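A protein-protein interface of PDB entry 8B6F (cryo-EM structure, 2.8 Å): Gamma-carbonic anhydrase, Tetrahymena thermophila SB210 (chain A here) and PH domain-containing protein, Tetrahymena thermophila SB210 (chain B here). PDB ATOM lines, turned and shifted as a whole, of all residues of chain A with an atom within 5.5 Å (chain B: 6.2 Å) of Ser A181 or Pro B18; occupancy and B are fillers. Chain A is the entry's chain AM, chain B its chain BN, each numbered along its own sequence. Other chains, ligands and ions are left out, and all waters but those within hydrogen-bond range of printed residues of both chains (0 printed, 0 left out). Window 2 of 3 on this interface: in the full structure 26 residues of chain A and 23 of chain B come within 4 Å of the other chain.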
ATOM      1  N   ASP A 144      -5.656   6.390  32.361  1.00  0.00           N
ATOM      2  CA  ASP A 144      -6.572   6.100  31.270  1.00  0.00           C
ATOM      3  C   ASP A 144      -6.240   4.725  30.691  1.00  0.00           C
ATOM      4  O   ASP A 144      -5.432   3.971  31.238  1.00  0.00           O
ATOM      5  CB  ASP A 144      -6.497   7.207  30.222  1.00  0.00           C
ATOM      6  CG  ASP A 144      -7.788   7.368  29.444  1.00  0.00           C
ATOM      7  OD1 ASP A 144      -8.752   6.625  29.720  1.00  0.00           O
ATOM      8  OD2 ASP A 144      -7.839   8.244  28.555  1.00  0.00           O
ATOM      9  N   GLU A 162      -2.966  10.186  30.666  1.00  0.00           N
ATOM     10  CA  GLU A 162      -3.898  10.021  29.564  1.00  0.00           C
ATOM     11  C   GLU A 162      -3.614   8.723  28.810  1.00  0.00           C
ATOM     12  O   GLU A 162      -2.648   8.007  29.084  1.00  0.00           O
ATOM     13  CB  GLU A 162      -3.822  11.221  28.621  1.00  0.00           C
ATOM     14  CG  GLU A 162      -4.211  12.531  29.286  1.00  0.00           C
ATOM     15  CD  GLU A 162      -4.280  13.687  28.310  1.00  0.00           C
ATOM     16  OE1 GLU A 162      -4.007  13.473  27.112  1.00  0.00           O
ATOM     17  OE2 GLU A 162      -4.605  14.813  28.743  1.00  0.00           O
ATOM     18  N   ARG A 163      -4.480   8.426  27.845  1.00  0.00           N
ATOM     19  CA  ARG A 163      -4.384   7.168  27.120  1.00  0.00           C
ATOM     20  C   ARG A 163      -3.055   7.063  26.383  1.00  0.00           C
ATOM     21  O   ARG A 163      -2.608   8.011  25.734  1.00  0.00           O
ATOM     22  CB  ARG A 163      -5.539   7.042  26.125  1.00  0.00           C
ATOM     23  CG  ARG A 163      -5.689   5.646  25.547  1.00  0.00           C
ATOM     24  CD  ARG A 163      -6.395   5.648  24.200  1.00  0.00           C
ATOM     25  NE  ARG A 163      -7.712   6.272  24.259  1.00  0.00           N
ATOM     26  CZ  ARG A 163      -7.993   7.499  23.840  1.00  0.00           C
ATOM     27  NH1 ARG A 163      -7.064   8.287  23.324  1.00  0.00           N
ATOM     28  NH2 ARG A 163      -9.241   7.946  23.936  1.00  0.00           N
ATOM     29  N   GLY A 164      -2.424   5.897  26.486  1.00  0.00           N
ATOM     30  CA  GLY A 164      -1.224   5.603  25.735  1.00  0.00           C
ATOM     31  C   GLY A 164       0.064   6.117  26.335  1.00  0.00           C
ATOM     32  O   GLY A 164       1.134   5.838  25.782  1.00  0.00           O
ATOM     33  N   SER A 165       0.006   6.851  27.439  1.00  0.00           N
ATOM     34  CA  SER A 165       1.225   7.353  28.053  1.00  0.00           C
ATOM     35  C   SER A 165       2.056   6.204  28.615  1.00  0.00           C
ATOM     36  O   SER A 165       1.527   5.193  29.082  1.00  0.00           O
ATOM     37  CB  SER A 165       0.893   8.355  29.159  1.00  0.00           C
ATOM     38  OG  SER A 165       0.038   7.780  30.130  1.00  0.00           O
ATOM     39  N   ILE A 179       0.229  13.613  32.565  1.00  0.00           N
ATOM     40  CA  ILE A 179       1.095  12.935  31.606  1.00  0.00           C
ATOM     41  C   ILE A 179       0.292  12.767  30.321  1.00  0.00           C
ATOM     42  O   ILE A 179      -0.535  11.849  30.229  1.00  0.00           O
ATOM     43  CB  ILE A 179       1.589  11.584  32.147  1.00  0.00           C
ATOM     44  CG1 ILE A 179       2.275  11.763  33.506  1.00  0.00           C
ATOM     45  CG2 ILE A 179       2.536  10.927  31.156  1.00  0.00           C
ATOM     46  CD1 ILE A 179       3.456  12.716  33.495  1.00  0.00           C
ATOM     47  N   PRO A 180       0.493  13.615  29.313  1.00  0.00           N
ATOM     48  CA  PRO A 180      -0.357  13.556  28.118  1.00  0.00           C
ATOM     49  C   PRO A 180      -0.278  12.207  27.422  1.00  0.00           C
ATOM     50  O   PRO A 180       0.531  11.336  27.751  1.00  0.00           O
ATOM     51  CB  PRO A 180       0.195  14.677  27.231  1.00  0.00           C
ATOM     52  CG  PRO A 180       0.854  15.612  28.174  1.00  0.00           C
ATOM     53  CD  PRO A 180       1.417  14.761  29.268  1.00  0.00           C
ATOM     54  N   SER A 181      -1.153  12.044  26.434  1.00  0.00           N
ATOM     55  CA  SER A 181      -1.288  10.786  25.717  1.00  0.00           C
ATOM     56  C   SER A 181      -0.141  10.575  24.740  1.00  0.00           C
ATOM     57  O   SER A 181       0.355  11.521  24.122  1.00  0.00           O
ATOM     58  CB  SER A 181      -2.615  10.755  24.960  1.00  0.00           C
ATOM     59  OG  SER A 181      -2.746  11.900  24.137  1.00  0.00           O
ATOM     60  N   GLY A 182       0.273   9.317  24.599  1.00  0.00           N
ATOM     61  CA  GLY A 182       1.232   8.949  23.578  1.00  0.00           C
ATOM     62  C   GLY A 182       2.635   9.463  23.791  1.00  0.00           C
ATOM     63  O   GLY A 182       3.379   9.606  22.819  1.00  0.00           O
ATOM     64  N   GLN A 183       3.020   9.752  25.031  1.00  0.00           N
ATOM     65  CA  GLN A 183       4.335  10.293  25.335  1.00  0.00           C
ATOM     66  C   GLN A 183       5.044   9.413  26.355  1.00  0.00           C
ATOM     67  O   GLN A 183       4.406   8.758  27.185  1.00  0.00           O
ATOM     68  CB  GLN A 183       4.234  11.725  25.869  1.00  0.00           C
ATOM     69  CG  GLN A 183       3.588  12.695  24.898  1.00  0.00           C
ATOM     70  CD  GLN A 183       3.450  14.084  25.477  1.00  0.00           C
ATOM     71  OE1 GLN A 183       3.841  14.335  26.615  1.00  0.00           O
ATOM     72  NE2 GLN A 183       2.891  14.998  24.694  1.00  0.00           N
ATOM     73  N   LEU B  16     -13.603   8.656  21.848  1.00  0.00           N
ATOM     74  CA  LEU B  16     -13.429  10.006  22.359  1.00  0.00           C
ATOM     75  C   LEU B  16     -11.951  10.379  22.410  1.00  0.00           C
ATOM     76  O   LEU B  16     -11.062   9.524  22.410  1.00  0.00           O
ATOM     77  CB  LEU B  16     -14.038  10.127  23.756  1.00  0.00           C
ATOM     78  CG  LEU B  16     -15.523   9.785  23.864  1.00  0.00           C
ATOM     79  CD1 LEU B  16     -15.958   9.771  25.316  1.00  0.00           C
ATOM     80  CD2 LEU B  16     -16.364  10.767  23.066  1.00  0.00           C
ATOM     81  N   THR B  17     -11.696  11.684  22.445  1.00  0.00           N
ATOM     82  CA  THR B  17     -10.345  12.178  22.625  1.00  0.00           C
ATOM     83  C   THR B  17      -9.863  11.863  24.039  1.00  0.00           C
ATOM     84  O   THR B  17     -10.671  11.663  24.948  1.00  0.00           O
ATOM     85  CB  THR B  17     -10.286  13.683  22.377  1.00  0.00           C
ATOM     86  OG1 THR B  17     -11.094  14.365  23.345  1.00  0.00           O
ATOM     87  CG2 THR B  17     -10.787  14.015  20.981  1.00  0.00           C
ATOM     88  N   PRO B  18      -8.545  11.807  24.250  1.00  0.00           N
ATOM     89  CA  PRO B  18      -8.055  11.504  25.606  1.00  0.00           C
ATOM     90  C   PRO B  18      -8.554  12.483  26.653  1.00  0.00           C
ATOM     91  O   PRO B  18      -8.833  12.075  27.787  1.00  0.00           O
ATOM     92  CB  PRO B  18      -6.527  11.553  25.446  1.00  0.00           C
ATOM     93  CG  PRO B  18      -6.286  12.304  24.185  1.00  0.00           C
ATOM     94  CD  PRO B  18      -7.442  12.000  23.296  1.00  0.00           C
ATOM     95  N   GLN B  19      -8.672  13.767  26.311  1.00  0.00           N
ATOM     96  CA  GLN B  19      -9.169  14.743  27.276  1.00  0.00           C
ATOM     97  C   GLN B  19     -10.603  14.422  27.678  1.00  0.00           C
ATOM     98  O   GLN B  19     -10.945  14.427  28.865  1.00  0.00           O
ATOM     99  CB  GLN B  19      -9.073  16.157  26.702  1.00  0.00           C
ATOM    100  CG  GLN B  19      -7.651  16.644  26.467  1.00  0.00           C
ATOM    101  CD  GLN B  19      -7.041  16.089  25.196  1.00  0.00           C
ATOM    102  OE1 GLN B  19      -7.728  15.478  24.379  1.00  0.00           O
ATOM    103  NE2 GLN B  19      -5.741  16.297  25.023  1.00  0.00           N
ATOM    104  N   GLU B  20     -11.461  14.153  26.694  1.00  0.00           N
ATOM    105  CA  GLU B  20     -12.845  13.808  26.998  1.00  0.00           C
ATOM    106  C   GLU B  20     -12.924  12.513  27.792  1.00  0.00           C
ATOM    107  O   GLU B  20     -13.747  12.382  28.705  1.00  0.00           O
ATOM    108  CB  GLU B  20     -13.657  13.701  25.707  1.00  0.00           C
ATOM    109  CG  GLU B  20     -13.762  15.014  24.947  1.00  0.00           C
ATOM    110  CD  GLU B  20     -14.447  14.858  23.604  1.00  0.00           C
ATOM    111  OE1 GLU B  20     -14.737  13.709  23.211  1.00  0.00           O
ATOM    112  OE2 GLU B  20     -14.697  15.886  22.940  1.00  0.00           O
ATOM    113  N   SER B  21     -12.081  11.537  27.452  1.00  0.00           N
ATOM    114  CA  SER B  21     -12.081  10.272  28.177  1.00  0.00           C
ATOM    115  C   SER B  21     -11.730  10.477  29.648  1.00  0.00           C
ATOM    116  O   SER B  21     -12.424   9.973  30.538  1.00  0.00           O
ATOM    117  CB  SER B  21     -11.100   9.303  27.517  1.00  0.00           C
ATOM    118  OG  SER B  21     -11.002   8.094  28.247  1.00  0.00           O
ATOM    119  N   VAL B  22     -10.658  11.221  29.926  1.00  0.00           N
ATOM    120  CA  VAL B  22     -10.255  11.433  31.314  1.00  0.00           C
ATOM    121  C   VAL B  22     -11.311  12.238  32.061  1.00  0.00           C
ATOM    122  O   VAL B  22     -11.593  11.973  33.235  1.00  0.00           O
ATOM    123  CB  VAL B  22      -8.870  12.104  31.392  1.00  0.00           C
ATOM    124  CG1 VAL B  22      -7.810  11.202  30.789  1.00  0.00           C
ATOM    125  CG2 VAL B  22      -8.874  13.459  30.705  1.00  0.00           C
ATOM    126  N   GLN B  23     -11.915  13.226  31.400  1.00  0.00           N
ATOM    127  CA  GLN B  23     -12.954  14.013  32.057  1.00  0.00           C
ATOM    128  C   GLN B  23     -14.155  13.149  32.415  1.00  0.00           C
ATOM    129  O   GLN B  23     -14.710  13.270  33.513  1.00  0.00           O
ATOM    130  CB  GLN B  23     -13.377  15.179  31.164  1.00  0.00           C
ATOM    131  CG  GLN B  23     -12.313  16.255  31.007  1.00  0.00           C
ATOM    132  CD  GLN B  23     -11.935  16.903  32.322  1.00  0.00           C
ATOM    133  OE1 GLN B  23     -12.702  16.875  33.285  1.00  0.00           O
ATOM    134  NE2 GLN B  23     -10.742  17.484  32.374  1.00  0.00           N
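The side-chain carboxylate (OD1) of Asp A144 lies within hydrogen-bond range of the side-chain hydroxyl (OG) of Ser B21 (3.1 Å). NH2 of Arg A163 sits at hydrogen-bond distance from O of Leu B16 (2.9 Å).
The backbone carbonyl oxygen of Glu A162 lies within hydrogen-bond range of the side-chain hydroxyl of Ser A165, at 2.9 Å. The backbone NH (N) of Ser A181 lies within hydrogen-bond range of the side-chain carboxylate (OE1) of Glu A162, at 3.3 Å. The backbone carbonyl oxygen (O) of Ile A179 is in hydrogen-bond range of the backbone NH (N) of Glu A162, at 3.0 Å. N of Glu B20 sits close to OG1 of Thr B17. N of Arg A163 sits close to OD2 of Asp A144 (3.4 Å). The backbone NH (N) of Gly A182 sits at hydrogen-bond distance from the backbone carbonyl oxygen (O) of Arg A163 (3.4 Å).
Of chain B, only Pro B18 comes within 4 Å of Ser A181. Of chain A, only Glu A162 (3.6 Å), Arg A163 (3.7 Å) and Ser A181 (3.6 Å) come within 4 Å of Pro B18. Of the printed residues of chain B, Glu A162 touches Pro B18 and Gln B19. Of the printed residues of chain B, Asp A144 touches Ser B21 (3.1 Å) and Val B22 (3.7 Å). Printed residues of chain A within 4 Å of Gln B19: Glu A162 (3.9 Å). Glu B20 touches none of the printed residues of chain A. Gly A164 touches none of the printed residues of chain B. The nearest residue of chain B that does not touch Ser A181 is Gln B19 (5.4 Å). The nearest residue of chain A that does not touch Pro B18 is Asp A144 (4.03 Å).
Among the printed residues, 8 pairs touch across the chains. Among the printed residues, no Asp or Glu carboxylate lies within 4 Å of a Lys or Arg side-chain nitrogen of the other chain.
Among the printed residues, pairs that only touch across the chains: Ser A181 with Pro B18 (3.6 Å), Glu A162 with Pro B18 (3.6 Å), Asp A144 with Val B22 (3.7 Å), Arg A163 with Pro B18 (3.7 Å), Glu A162 with Gln B19 (3.9 Å) and Arg A163 with Thr B17 (3.97 Å).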
